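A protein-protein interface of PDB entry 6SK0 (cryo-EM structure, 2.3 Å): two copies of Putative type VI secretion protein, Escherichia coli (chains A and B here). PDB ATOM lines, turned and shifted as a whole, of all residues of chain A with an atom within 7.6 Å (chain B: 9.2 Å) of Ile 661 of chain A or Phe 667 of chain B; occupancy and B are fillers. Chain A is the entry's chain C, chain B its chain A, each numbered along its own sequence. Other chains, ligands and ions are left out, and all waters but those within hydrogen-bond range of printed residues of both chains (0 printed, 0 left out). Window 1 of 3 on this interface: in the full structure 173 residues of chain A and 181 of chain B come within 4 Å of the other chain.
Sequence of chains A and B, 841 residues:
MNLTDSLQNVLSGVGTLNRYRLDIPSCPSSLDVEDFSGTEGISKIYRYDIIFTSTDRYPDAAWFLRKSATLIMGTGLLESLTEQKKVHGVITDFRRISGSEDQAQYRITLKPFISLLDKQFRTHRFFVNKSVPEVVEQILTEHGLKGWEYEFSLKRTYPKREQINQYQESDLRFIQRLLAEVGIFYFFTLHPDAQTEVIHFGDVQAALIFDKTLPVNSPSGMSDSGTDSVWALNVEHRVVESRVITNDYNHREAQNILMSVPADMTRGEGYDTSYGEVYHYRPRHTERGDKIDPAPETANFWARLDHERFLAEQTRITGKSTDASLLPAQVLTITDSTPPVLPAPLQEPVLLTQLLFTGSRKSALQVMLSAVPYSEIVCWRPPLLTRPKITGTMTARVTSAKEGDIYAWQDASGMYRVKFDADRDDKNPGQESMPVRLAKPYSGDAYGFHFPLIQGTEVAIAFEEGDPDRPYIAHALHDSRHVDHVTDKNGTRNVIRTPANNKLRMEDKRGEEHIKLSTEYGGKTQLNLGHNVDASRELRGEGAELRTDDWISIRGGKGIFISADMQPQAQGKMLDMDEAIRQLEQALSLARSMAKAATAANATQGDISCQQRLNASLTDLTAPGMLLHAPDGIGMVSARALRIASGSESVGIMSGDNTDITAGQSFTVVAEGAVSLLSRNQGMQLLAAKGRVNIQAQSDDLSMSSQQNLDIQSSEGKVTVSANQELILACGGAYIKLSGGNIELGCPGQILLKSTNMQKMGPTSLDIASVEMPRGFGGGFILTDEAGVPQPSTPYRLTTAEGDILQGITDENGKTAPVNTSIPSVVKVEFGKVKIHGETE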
ATOM      1  N   ILE A 653      -4.321 -10.468  27.609  1.00  0.00           N
ATOM      2  CA  ILE A 653      -3.122  -9.992  26.945  1.00  0.00           C
ATOM      3  C   ILE A 653      -3.564  -9.237  25.706  1.00  0.00           C
ATOM      4  O   ILE A 653      -4.226  -9.804  24.830  1.00  0.00           O
ATOM      5  CB  ILE A 653      -2.166 -11.137  26.594  1.00  0.00           C
ATOM      6  CG1 ILE A 653      -1.754 -11.872  27.864  1.00  0.00           C
ATOM      7  CG2 ILE A 653      -0.959 -10.613  25.849  1.00  0.00           C
ATOM      8  CD1 ILE A 653      -1.037 -13.140  27.611  1.00  0.00           C
ATOM      9  N   SER A 655      -2.256  -6.503  22.618  1.00  0.00           N
ATOM     10  CA  SER A 655      -1.142  -5.892  21.921  1.00  0.00           C
ATOM     11  C   SER A 655      -1.702  -5.114  20.748  1.00  0.00           C
ATOM     12  O   SER A 655      -2.516  -5.644  19.991  1.00  0.00           O
ATOM     13  CB  SER A 655      -0.131  -6.944  21.451  1.00  0.00           C
ATOM     14  OG  SER A 655      -0.726  -7.862  20.554  1.00  0.00           O
ATOM     15  N   ASP A 657       0.278  -4.286  18.395  1.00  0.00           N
ATOM     16  CA  ASP A 657       1.000  -5.097  17.428  1.00  0.00           C
ATOM     17  C   ASP A 657       0.791  -6.581  17.739  1.00  0.00           C
ATOM     18  O   ASP A 657      -0.267  -6.992  18.214  1.00  0.00           O
ATOM     19  CB  ASP A 657       2.465  -4.674  17.390  1.00  0.00           C
ATOM     20  CG  ASP A 657       2.681  -3.449  16.541  1.00  0.00           C
ATOM     21  OD1 ASP A 657       3.795  -2.883  16.568  1.00  0.00           O
ATOM     22  OD2 ASP A 657       1.731  -3.045  15.843  1.00  0.00           O
ATOM     23  N   ASN A 658       1.746  -7.404  17.337  1.00  0.00           N
ATOM     24  CA  ASN A 658       1.710  -8.835  17.565  1.00  0.00           C
ATOM     25  C   ASN A 658       1.695  -9.206  19.048  1.00  0.00           C
ATOM     26  O   ASN A 658       2.131  -8.462  19.920  1.00  0.00           O
ATOM     27  CB  ASN A 658       2.921  -9.490  16.921  1.00  0.00           C
ATOM     28  CG  ASN A 658       2.833  -9.555  15.430  1.00  0.00           C
ATOM     29  OD1 ASN A 658       1.850  -9.151  14.833  1.00  0.00           O
ATOM     30  ND2 ASN A 658       3.872 -10.081  14.814  1.00  0.00           N
ATOM     31  N   THR A 659       1.186 -10.397  19.319  1.00  0.00           N
ATOM     32  CA  THR A 659       1.450 -11.119  20.554  1.00  0.00           C
ATOM     33  C   THR A 659       2.249 -12.349  20.160  1.00  0.00           C
ATOM     34  O   THR A 659       1.710 -13.262  19.531  1.00  0.00           O
ATOM     35  CB  THR A 659       0.164 -11.508  21.278  1.00  0.00           C
ATOM     36  OG1 THR A 659      -0.522 -10.332  21.714  1.00  0.00           O
ATOM     37  CG2 THR A 659       0.471 -12.387  22.473  1.00  0.00           C
ATOM     38  N   ASP A 660       3.530 -12.362  20.497  1.00  0.00           N
ATOM     39  CA  ASP A 660       4.445 -13.425  20.099  1.00  0.00           C
ATOM     40  C   ASP A 660       4.747 -14.296  21.302  1.00  0.00           C
ATOM     41  O   ASP A 660       5.095 -13.791  22.370  1.00  0.00           O
ATOM     42  CB  ASP A 660       5.762 -12.878  19.542  1.00  0.00           C
ATOM     43  CG  ASP A 660       5.561 -11.716  18.620  1.00  0.00           C
ATOM     44  OD1 ASP A 660       6.517 -11.291  17.932  1.00  0.00           O
ATOM     45  OD2 ASP A 660       4.461 -11.172  18.618  1.00  0.00           O
ATOM     46  N   ILE A 661       4.623 -15.597  21.123  1.00  0.00           N
ATOM     47  CA  ILE A 661       5.030 -16.560  22.126  1.00  0.00           C
ATOM     48  C   ILE A 661       6.140 -17.397  21.525  1.00  0.00           C
ATOM     49  O   ILE A 661       5.976 -17.984  20.450  1.00  0.00           O
ATOM     50  CB  ILE A 661       3.864 -17.432  22.601  1.00  0.00           C
ATOM     51  CG1 ILE A 661       2.805 -16.559  23.266  1.00  0.00           C
ATOM     52  CG2 ILE A 661       4.366 -18.500  23.540  1.00  0.00           C
ATOM     53  CD1 ILE A 661       1.602 -17.310  23.711  1.00  0.00           C
ATOM     54  N   THR A 662       7.265 -17.439  22.214  1.00  0.00           N
ATOM     55  CA  THR A 662       8.437 -18.177  21.784  1.00  0.00           C
ATOM     56  C   THR A 662       8.816 -19.131  22.906  1.00  0.00           C
ATOM     57  O   THR A 662       9.298 -18.701  23.957  1.00  0.00           O
ATOM     58  CB  THR A 662       9.576 -17.216  21.448  1.00  0.00           C
ATOM     59  OG1 THR A 662       9.233 -16.473  20.276  1.00  0.00           O
ATOM     60  CG2 THR A 662      10.828 -17.960  21.186  1.00  0.00           C
ATOM     61  N   ALA A 663       8.571 -20.415  22.697  1.00  0.00           N
ATOM     62  CA  ALA A 663       8.815 -21.433  23.704  1.00  0.00           C
ATOM     63  C   ALA A 663      10.055 -22.220  23.323  1.00  0.00           C
ATOM     64  O   ALA A 663      10.111 -22.817  22.245  1.00  0.00           O
ATOM     65  CB  ALA A 663       7.613 -22.364  23.857  1.00  0.00           C
ATOM     66  N   GLY A 664      11.046 -22.213  24.208  1.00  0.00           N
ATOM     67  CA  GLY A 664      12.199 -23.062  24.008  1.00  0.00           C
ATOM     68  C   GLY A 664      11.872 -24.537  24.075  1.00  0.00           C
ATOM     69  O   GLY A 664      12.621 -25.357  23.548  1.00  0.00           O
ATOM     70  N   SER A 666       7.878 -26.013  24.622  1.00  0.00           N
ATOM     71  CA  SER A 666       6.567 -26.326  24.076  1.00  0.00           C
ATOM     72  C   SER A 666       5.568 -25.266  24.493  1.00  0.00           C
ATOM     73  O   SER A 666       5.680 -24.660  25.554  1.00  0.00           O
ATOM     74  CB  SER A 666       6.060 -27.703  24.524  1.00  0.00           C
ATOM     75  OG  SER A 666       6.583 -28.740  23.722  1.00  0.00           O
ATOM     76  N   PHE A 667       4.590 -25.055  23.642  1.00  0.00           N
ATOM     77  CA  PHE A 667       3.464 -24.193  23.944  1.00  0.00           C
ATOM     78  C   PHE A 667       2.260 -25.088  24.173  1.00  0.00           C
ATOM     79  O   PHE A 667       1.795 -25.762  23.250  1.00  0.00           O
ATOM     80  CB  PHE A 667       3.212 -23.196  22.822  1.00  0.00           C
ATOM     81  CG  PHE A 667       2.002 -22.351  23.033  1.00  0.00           C
ATOM     82  CD1 PHE A 667       1.967 -21.422  24.052  1.00  0.00           C
ATOM     83  CD2 PHE A 667       0.895 -22.487  22.223  1.00  0.00           C
ATOM     84  CE1 PHE A 667       0.863 -20.645  24.252  1.00  0.00           C
ATOM     85  CE2 PHE A 667      -0.215 -21.703  22.418  1.00  0.00           C
ATOM     86  CZ  PHE A 667      -0.228 -20.775  23.434  1.00  0.00           C
ATOM     87  N   THR A 668       1.772 -25.112  25.402  1.00  0.00           N
ATOM     88  CA  THR A 668       0.650 -25.957  25.767  1.00  0.00           C
ATOM     89  C   THR A 668      -0.473 -25.088  26.299  1.00  0.00           C
ATOM     90  O   THR A 668      -0.239 -24.172  27.091  1.00  0.00           O
ATOM     91  CB  THR A 668       1.050 -27.020  26.801  1.00  0.00           C
ATOM     92  OG1 THR A 668       1.269 -26.408  28.076  1.00  0.00           O
ATOM     93  CG2 THR A 668       2.317 -27.741  26.369  1.00  0.00           C
ATOM     94  N   VAL A 669      -1.681 -25.365  25.843  1.00  0.00           N
ATOM     95  CA  VAL A 669      -2.884 -24.728  26.340  1.00  0.00           C
ATOM     96  C   VAL A 669      -3.826 -25.827  26.788  1.00  0.00           C
ATOM     97  O   VAL A 669      -4.129 -26.744  26.019  1.00  0.00           O
ATOM     98  CB  VAL A 669      -3.559 -23.844  25.280  1.00  0.00           C
ATOM     99  CG1 VAL A 669      -4.900 -23.367  25.786  1.00  0.00           C
ATOM    100  CG2 VAL A 669      -2.680 -22.682  24.905  1.00  0.00           C
ATOM    101  N   LEU A 677      -9.354 -19.737  18.389  1.00  0.00           N
ATOM    102  CA  LEU A 677      -8.381 -18.922  17.680  1.00  0.00           C
ATOM    103  C   LEU A 677      -9.073 -18.290  16.488  1.00  0.00           C
ATOM    104  O   LEU A 677      -9.515 -18.995  15.576  1.00  0.00           O
ATOM    105  CB  LEU A 677      -7.180 -19.749  17.227  1.00  0.00           C
ATOM    106  CG  LEU A 677      -6.506 -20.661  18.246  1.00  0.00           C
ATOM    107  CD1 LEU A 677      -5.303 -21.321  17.614  1.00  0.00           C
ATOM    108  CD2 LEU A 677      -6.103 -19.889  19.480  1.00  0.00           C
ATOM    109  N   LEU A 678      -9.172 -16.971  16.499  1.00  0.00           N
ATOM    110  CA  LEU A 678      -9.782 -16.227  15.413  1.00  0.00           C
ATOM    111  C   LEU A 678      -8.755 -15.284  14.810  1.00  0.00           C
ATOM    112  O   LEU A 678      -8.244 -14.391  15.491  1.00  0.00           O
ATOM    113  CB  LEU A 678     -11.009 -15.454  15.886  1.00  0.00           C
ATOM    114  CG  LEU A 678     -11.591 -14.505  14.840  1.00  0.00           C
ATOM    115  CD1 LEU A 678     -12.037 -15.247  13.583  1.00  0.00           C
ATOM    116  CD2 LEU A 678     -12.726 -13.722  15.436  1.00  0.00           C
ATOM    117  N   SER A 679      -8.451 -15.494  13.545  1.00  0.00           N
ATOM    118  CA  SER A 679      -7.700 -14.544  12.749  1.00  0.00           C
ATOM    119  C   SER A 679      -8.692 -13.731  11.933  1.00  0.00           C
ATOM    120  O   SER A 679      -9.613 -14.289  11.335  1.00  0.00           O
ATOM    121  CB  SER A 679      -6.705 -15.266  11.845  1.00  0.00           C
ATOM    122  OG  SER A 679      -6.210 -14.408  10.846  1.00  0.00           O
ATOM    123  N   GLY A 683      -5.515 -14.861   7.848  1.00  0.00           N
ATOM    124  CA  GLY A 683      -5.583 -16.295   7.888  1.00  0.00           C
ATOM    125  C   GLY A 683      -4.845 -16.912   9.062  1.00  0.00           C
ATOM    126  O   GLY A 683      -4.349 -16.252   9.965  1.00  0.00           O
ATOM    127  N   GLN A 685      -2.154 -20.163  10.201  1.00  0.00           N
ATOM    128  CA  GLN A 685      -1.170 -21.182   9.877  1.00  0.00           C
ATOM    129  C   GLN A 685      -0.960 -22.045  11.108  1.00  0.00           C
ATOM    130  O   GLN A 685      -0.557 -21.543  12.161  1.00  0.00           O
ATOM    131  CB  GLN A 685       0.146 -20.565   9.410  1.00  0.00           C
ATOM    132  CG  GLN A 685       0.007 -19.606   8.255  1.00  0.00           C
ATOM    133  CD  GLN A 685      -0.264 -18.191   8.716  1.00  0.00           C
ATOM    134  OE1 GLN A 685       0.432 -17.671   9.588  1.00  0.00           O
ATOM    135  NE2 GLN A 685      -1.285 -17.562   8.145  1.00  0.00           N
ATOM    136  N   ILE B 644       7.626 -10.816  28.783  1.00  0.00           N
ATOM    137  CA  ILE B 644       7.574 -11.743  29.893  1.00  0.00           C
ATOM    138  C   ILE B 644       8.419 -12.930  29.472  1.00  0.00           C
ATOM    139  O   ILE B 644       8.081 -13.629  28.511  1.00  0.00           O
ATOM    140  CB  ILE B 644       6.138 -12.157  30.226  1.00  0.00           C
ATOM    141  CG1 ILE B 644       5.375 -10.969  30.807  1.00  0.00           C
ATOM    142  CG2 ILE B 644       6.121 -13.310  31.188  1.00  0.00           C
ATOM    143  CD1 ILE B 644       4.570 -10.242  29.812  1.00  0.00           C
ATOM    144  N   VAL B 651       7.088 -20.267  31.368  1.00  0.00           N
ATOM    145  CA  VAL B 651       6.142 -19.206  31.655  1.00  0.00           C
ATOM    146  C   VAL B 651       4.778 -19.855  31.790  1.00  0.00           C
ATOM    147  O   VAL B 651       4.289 -20.498  30.855  1.00  0.00           O
ATOM    148  CB  VAL B 651       6.154 -18.129  30.561  1.00  0.00           C
ATOM    149  CG1 VAL B 651       5.049 -17.129  30.789  1.00  0.00           C
ATOM    150  CG2 VAL B 651       7.511 -17.446  30.509  1.00  0.00           C
ATOM    151  N   ILE B 653       0.785 -19.253  32.583  1.00  0.00           N
ATOM    152  CA  ILE B 653      -0.348 -18.349  32.664  1.00  0.00           C
ATOM    153  C   ILE B 653      -1.545 -19.167  33.105  1.00  0.00           C
ATOM    154  O   ILE B 653      -1.934 -20.125  32.428  1.00  0.00           O
ATOM    155  CB  ILE B 653      -0.612 -17.640  31.331  1.00  0.00           C
ATOM    156  CG1 ILE B 653       0.617 -16.837  30.922  1.00  0.00           C
ATOM    157  CG2 ILE B 653      -1.833 -16.754  31.434  1.00  0.00           C
ATOM    158  CD1 ILE B 653       0.557 -16.322  29.536  1.00  0.00           C
ATOM    159  N   THR B 659      -8.424 -17.077  29.497  1.00  0.00           N
ATOM    160  CA  THR B 659      -7.181 -16.424  29.113  1.00  0.00           C
ATOM    161  C   THR B 659      -7.407 -15.882  27.713  1.00  0.00           C
ATOM    162  O   THR B 659      -7.507 -16.653  26.758  1.00  0.00           O
ATOM    163  CB  THR B 659      -5.995 -17.384  29.145  1.00  0.00           C
ATOM    164  OG1 THR B 659      -5.752 -17.811  30.488  1.00  0.00           O
ATOM    165  CG2 THR B 659      -4.753 -16.714  28.594  1.00  0.00           C
ATOM    166  N   ASP B 660      -7.519 -14.566  27.593  1.00  0.00           N
ATOM    167  CA  ASP B 660      -7.838 -13.907  26.334  1.00  0.00           C
ATOM    168  C   ASP B 660      -6.589 -13.239  25.792  1.00  0.00           C
ATOM    169  O   ASP B 660      -5.909 -12.508  26.513  1.00  0.00           O
ATOM    170  CB  ASP B 660      -8.934 -12.852  26.492  1.00  0.00           C
ATOM    171  CG  ASP B 660     -10.056 -13.311  27.370  1.00  0.00           C
ATOM    172  OD1 ASP B 660     -11.114 -12.643  27.435  1.00  0.00           O
ATOM    173  OD2 ASP B 660      -9.871 -14.310  28.058  1.00  0.00           O
ATOM    174  N   ILE B 661      -6.300 -13.482  24.529  1.00  0.00           N
ATOM    175  CA  ILE B 661      -5.236 -12.792  23.830  1.00  0.00           C
ATOM    176  C   ILE B 661      -5.870 -12.013  22.697  1.00  0.00           C
ATOM    177  O   ILE B 661      -6.593 -12.579  21.868  1.00  0.00           O
ATOM    178  CB  ILE B 661      -4.161 -13.753  23.315  1.00  0.00           C
ATOM    179  CG1 ILE B 661      -3.496 -14.460  24.494  1.00  0.00           C
ATOM    180  CG2 ILE B 661      -3.150 -13.002  22.486  1.00  0.00           C
ATOM    181  CD1 ILE B 661      -2.473 -15.459  24.092  1.00  0.00           C
ATOM    182  N   THR B 662      -5.609 -10.720  22.671  1.00  0.00           N
ATOM    183  CA  THR B 662      -6.141  -9.816  21.670  1.00  0.00           C
ATOM    184  C   THR B 662      -4.964  -9.109  21.016  1.00  0.00           C
ATOM    185  O   THR B 662      -4.320  -8.262  21.638  1.00  0.00           O
ATOM    186  CB  THR B 662      -7.114  -8.828  22.310  1.00  0.00           C
ATOM    187  OG1 THR B 662      -8.281  -9.529  22.744  1.00  0.00           O
ATOM    188  CG2 THR B 662      -7.522  -7.790  21.336  1.00  0.00           C
ATOM    189  N   ALA B 663      -4.668  -9.476  19.780  1.00  0.00           N
ATOM    190  CA  ALA B 663      -3.530  -8.939  19.054  1.00  0.00           C
ATOM    191  C   ALA B 663      -4.027  -7.958  18.008  1.00  0.00           C
ATOM    192  O   ALA B 663      -4.819  -8.319  17.136  1.00  0.00           O
ATOM    193  CB  ALA B 663      -2.711 -10.050  18.401  1.00  0.00           C
ATOM    194  N   GLY B 664      -3.562  -6.716  18.106  1.00  0.00           N
ATOM    195  CA  GLY B 664      -3.849  -5.755  17.066  1.00  0.00           C
ATOM    196  C   GLY B 664      -3.219  -6.107  15.737  1.00  0.00           C
ATOM    197  O   GLY B 664      -3.676  -5.637  14.696  1.00  0.00           O
ATOM    198  N   GLN B 665      -2.161  -6.914  15.741  1.00  0.00           N
ATOM    199  CA  GLN B 665      -1.683  -7.446  14.477  1.00  0.00           C
ATOM    200  C   GLN B 665      -1.804  -8.964  14.406  1.00  0.00           C
ATOM    201  O   GLN B 665      -2.774  -9.463  13.850  1.00  0.00           O
ATOM    202  CB  GLN B 665      -0.233  -7.017  14.257  1.00  0.00           C
ATOM    203  CG  GLN B 665      -0.063  -5.592  13.790  1.00  0.00           C
ATOM    204  CD  GLN B 665      -0.824  -5.293  12.518  1.00  0.00           C
ATOM    205  OE1 GLN B 665      -0.921  -6.132  11.630  1.00  0.00           O
ATOM    206  NE2 GLN B 665      -1.362  -4.092  12.423  1.00  0.00           N
ATOM    207  N   SER B 666      -0.970  -9.710  15.112  1.00  0.00           N
ATOM    208  CA  SER B 666      -0.932 -11.145  14.868  1.00  0.00           C
ATOM    209  C   SER B 666      -0.568 -11.874  16.144  1.00  0.00           C
ATOM    210  O   SER B 666       0.152 -11.361  16.995  1.00  0.00           O
ATOM    211  CB  SER B 666       0.064 -11.524  13.765  1.00  0.00           C
ATOM    212  OG  SER B 666      -0.496 -11.375  12.479  1.00  0.00           O
ATOM    213  N   PHE B 667      -1.075 -13.080  16.262  1.00  0.00           N
ATOM    214  CA  PHE B 667      -0.710 -13.979  17.340  1.00  0.00           C
ATOM    215  C   PHE B 667       0.166 -15.064  16.742  1.00  0.00           C
ATOM    216  O   PHE B 667      -0.294 -15.861  15.920  1.00  0.00           O
ATOM    217  CB  PHE B 667      -1.942 -14.566  18.013  1.00  0.00           C
ATOM    218  CG  PHE B 667      -1.625 -15.578  19.062  1.00  0.00           C
ATOM    219  CD1 PHE B 667      -0.997 -15.201  20.231  1.00  0.00           C
ATOM    220  CD2 PHE B 667      -1.946 -16.906  18.881  1.00  0.00           C
ATOM    221  CE1 PHE B 667      -0.702 -16.121  21.195  1.00  0.00           C
ATOM    222  CE2 PHE B 667      -1.657 -17.833  19.853  1.00  0.00           C
ATOM    223  CZ  PHE B 667      -1.037 -17.436  21.016  1.00  0.00           C
ATOM    224  N   THR B 668       1.428 -15.082  17.135  1.00  0.00           N
ATOM    225  CA  THR B 668       2.384 -16.039  16.610  1.00  0.00           C
ATOM    226  C   THR B 668       2.952 -16.854  17.758  1.00  0.00           C
ATOM    227  O   THR B 668       3.295 -16.308  18.808  1.00  0.00           O
ATOM    228  CB  THR B 668       3.510 -15.350  15.825  1.00  0.00           C
ATOM    229  OG1 THR B 668       4.385 -14.659  16.724  1.00  0.00           O
ATOM    230  CG2 THR B 668       2.939 -14.357  14.825  1.00  0.00           C
ATOM    231  N   VAL B 669       3.025 -18.157  17.556  1.00  0.00           N
ATOM    232  CA  VAL B 669       3.660 -19.070  18.485  1.00  0.00           C
ATOM    233  C   VAL B 669       4.711 -19.843  17.715  1.00  0.00           C
ATOM    234  O   VAL B 669       4.410 -20.447  16.680  1.00  0.00           O
ATOM    235  CB  VAL B 669       2.656 -20.035  19.135  1.00  0.00           C
ATOM    236  CG1 VAL B 669       3.393 -21.082  19.937  1.00  0.00           C
ATOM    237  CG2 VAL B 669       1.671 -19.292  19.996  1.00  0.00           C
ATOM    238  N   VAL B 670       5.936 -19.817  18.208  1.00  0.00           N
ATOM    239  CA  VAL B 670       6.966 -20.734  17.763  1.00  0.00           C
ATOM    240  C   VAL B 670       7.414 -21.511  18.985  1.00  0.00           C
ATOM    241  O   VAL B 670       7.943 -20.933  19.939  1.00  0.00           O
ATOM    242  CB  VAL B 670       8.147 -20.024  17.091  1.00  0.00           C
ATOM    243  CG1 VAL B 670       9.089 -21.051  16.495  1.00  0.00           C
ATOM    244  CG2 VAL B 670       7.652 -19.087  16.035  1.00  0.00           C
ATOM    245  N   ALA B 671       7.174 -22.808  18.970  1.00  0.00           N
ATOM    246  CA  ALA B 671       7.642 -23.705  20.008  1.00  0.00           C
ATOM    247  C   ALA B 671       8.708 -24.605  19.416  1.00  0.00           C
ATOM    248  O   ALA B 671       8.531 -25.147  18.322  1.00  0.00           O
ATOM    249  CB  ALA B 671       6.497 -24.533  20.587  1.00  0.00           C
ATOM    250  N   GLU B 672       9.817 -24.746  20.130  1.00  0.00           N
ATOM    251  CA  GLU B 672      10.857 -25.658  19.684  1.00  0.00           C
ATOM    252  C   GLU B 672      10.366 -27.096  19.713  1.00  0.00           C
ATOM    253  O   GLU B 672      10.686 -27.885  18.821  1.00  0.00           O
ATOM    254  CB  GLU B 672      12.102 -25.487  20.545  1.00  0.00           C
ATOM    255  CG  GLU B 672      13.280 -26.309  20.090  1.00  0.00           C
ATOM    256  CD  GLU B 672      13.780 -25.900  18.722  1.00  0.00           C
ATOM    257  OE1 GLU B 672      13.658 -24.712  18.370  1.00  0.00           O
ATOM    258  OE2 GLU B 672      14.297 -26.768  17.994  1.00  0.00           O
ATOM    259  N   ALA B 674       6.617 -28.985  20.996  1.00  0.00           N
ATOM    260  CA  ALA B 674       5.266 -29.212  20.523  1.00  0.00           C
ATOM    261  C   ALA B 674       4.397 -27.980  20.732  1.00  0.00           C
ATOM    262  O   ALA B 674       4.679 -27.128  21.573  1.00  0.00           O
ATOM    263  CB  ALA B 674       4.637 -30.413  21.228  1.00  0.00           C
ATOM    264  N   VAL B 675       3.344 -27.893  19.940  1.00  0.00           N
ATOM    265  CA  VAL B 675       2.234 -26.991  20.190  1.00  0.00           C
ATOM    266  C   VAL B 675       1.036 -27.861  20.516  1.00  0.00           C
ATOM    267  O   VAL B 675       0.651 -28.725  19.722  1.00  0.00           O
ATOM    268  CB  VAL B 675       1.955 -26.078  18.991  1.00  0.00           C
ATOM    269  CG1 VAL B 675       0.672 -25.306  19.200  1.00  0.00           C
ATOM    270  CG2 VAL B 675       3.125 -25.145  18.755  1.00  0.00           C
ATOM    271  N   LEU B 677      -2.896 -27.700  22.030  1.00  0.00           N
ATOM    272  CA  LEU B 677      -4.099 -27.006  22.454  1.00  0.00           C
ATOM    273  C   LEU B 677      -5.136 -28.045  22.832  1.00  0.00           C
ATOM    274  O   LEU B 677      -5.584 -28.818  21.979  1.00  0.00           O
ATOM    275  CB  LEU B 677      -4.636 -26.087  21.357  1.00  0.00           C
ATOM    276  CG  LEU B 677      -3.659 -25.141  20.669  1.00  0.00           C
ATOM    277  CD1 LEU B 677      -4.406 -24.276  19.680  1.00  0.00           C
ATOM    278  CD2 LEU B 677      -2.931 -24.286  21.679  1.00  0.00           C
ATOM    279  N   LEU B 686     -11.010 -22.979  15.322  1.00  0.00           N
ATOM    280  CA  LEU B 686      -9.855 -22.427  14.629  1.00  0.00           C
ATOM    281  C   LEU B 686     -10.405 -21.757  13.379  1.00  0.00           C
ATOM    282  O   LEU B 686     -10.706 -22.419  12.384  1.00  0.00           O
ATOM    283  CB  LEU B 686      -8.833 -23.515  14.322  1.00  0.00           C
ATOM    284  CG  LEU B 686      -8.542 -24.440  15.512  1.00  0.00           C
ATOM    285  CD1 LEU B 686      -7.816 -25.703  15.093  1.00  0.00           C
ATOM    286  CD2 LEU B 686      -7.752 -23.716  16.586  1.00  0.00           C
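Hydrophobic or aromatic side chains of chain B that line the printed part of chain A: Ile 661, Ala 663, Phe 667, Val 669, Ala 671, Ala 674, Leu 677 and Leu 686. Printed residues of chain A that touch a printed residue of chain B: Ile 653, Ser 655, Asp 657, Asn 658, Thr 659, Asp 660, Ile 661, Thr 662, Ala 663, Gly 664, Ser 666, Phe 667, Val 669 and Leu 677. Along chain A the printed residues that touch a printed residue of chain B span positions 653 to 677. Among the printed residues, no Asp or Glu carboxylate lies within 4 Å of a Lys or Arg side-chain nitrogen of the other chain.
Of chain A, only Thr 659 (3.3 Å) and Ile 661 (3.6 Å) come within 4 Å of Phe 667 of chain B. Of chain B, only Val 670 comes within 4 Å of Thr 662 of chain A. Of the printed residues of chain B, Thr 659 of chain A touches Ile 661, Ala 663, Ser 666, Phe 667 and Thr 668. Of the printed residues of chain B, Ala 663 of chain A touches Val 670 (2.9 Å), Ala 671 (3.4 Å) and Glu 672 (2.9 Å). The nearest residue of chain B that does not touch Ile 661 of chain A is Ile 661 of chain B (4.5 Å). The nearest residue of chain A that does not touch Phe 667 of chain B is Phe 667 of chain A (4.2 Å).
N of Thr 662 of chain B is in hydrogen-bond range of O of Ile 653 of chain A, 2.7 Å away. N of Ser 666 of chain B is in hydrogen-bond range of OD1 of Asn 658 of chain A (2.9 Å). OG of Ser 666 of chain A is in hydrogen-bond range of N of Ala 674 of chain B, 2.7 Å away. N of Val 670 of chain B is in hydrogen-bond range of O of Ile 661 of chain A. N of Gln 665 of chain B lies within hydrogen-bond range of O of Asp 657 of chain A, 3.1 Å away. The backbone NH of Thr 668 of chain B lies within hydrogen-bond range of the backbone carbonyl oxygen of Thr 659 of chain A, 3.0 Å away. O of Thr 668 of chain B is in hydrogen-bond range of N of Ile 661 of chain A. N of Phe 667 of chain A lies within hydrogen-bond range of O of Ala 674 of chain B. The backbone carbonyl oxygen (O) of Ala 663 of chain A lies within hydrogen-bond range of the backbone NH (N) of Glu 672 of chain B, at 2.9 Å. N of Gly 664 of chain B sits at hydrogen-bond distance from O of Ser 655 of chain A, 2.4 Å away. The backbone NH of Ser 655 of chain A sits at hydrogen-bond distance from the backbone carbonyl oxygen of Thr 662 of chain B, at 2.9 Å. The backbone NH (N) of Thr 659 of chain A sits at hydrogen-bond distance from the backbone carbonyl oxygen (O) of Ser 666 of chain B, at 2.7 Å. The backbone carbonyl oxygen (O) of Val 670 of chain B sits at hydrogen-bond distance from the backbone NH (N) of Ala 663 of chain A (2.9 Å). N of Gly 664 of chain B sits at hydrogen-bond distance from O of Asp 657 of chain A, at 3.3 Å. The backbone carbonyl oxygen (O) of Asp 660 of chain B is in hydrogen-bond range of the backbone NH (N) of Ile 653 of chain A.
The side-chain hydroxyl (OG) of Ser 655 of chain A is in hydrogen-bond range of the backbone carbonyl oxygen (O) of Asn 658 of chain A (3.0 Å).
Ile 661 of chain A touches Phe 667 of chain B, but with the chains exchanged Phe 667 of chain A does not touch Ile 661 of chain B (5.8 Å).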
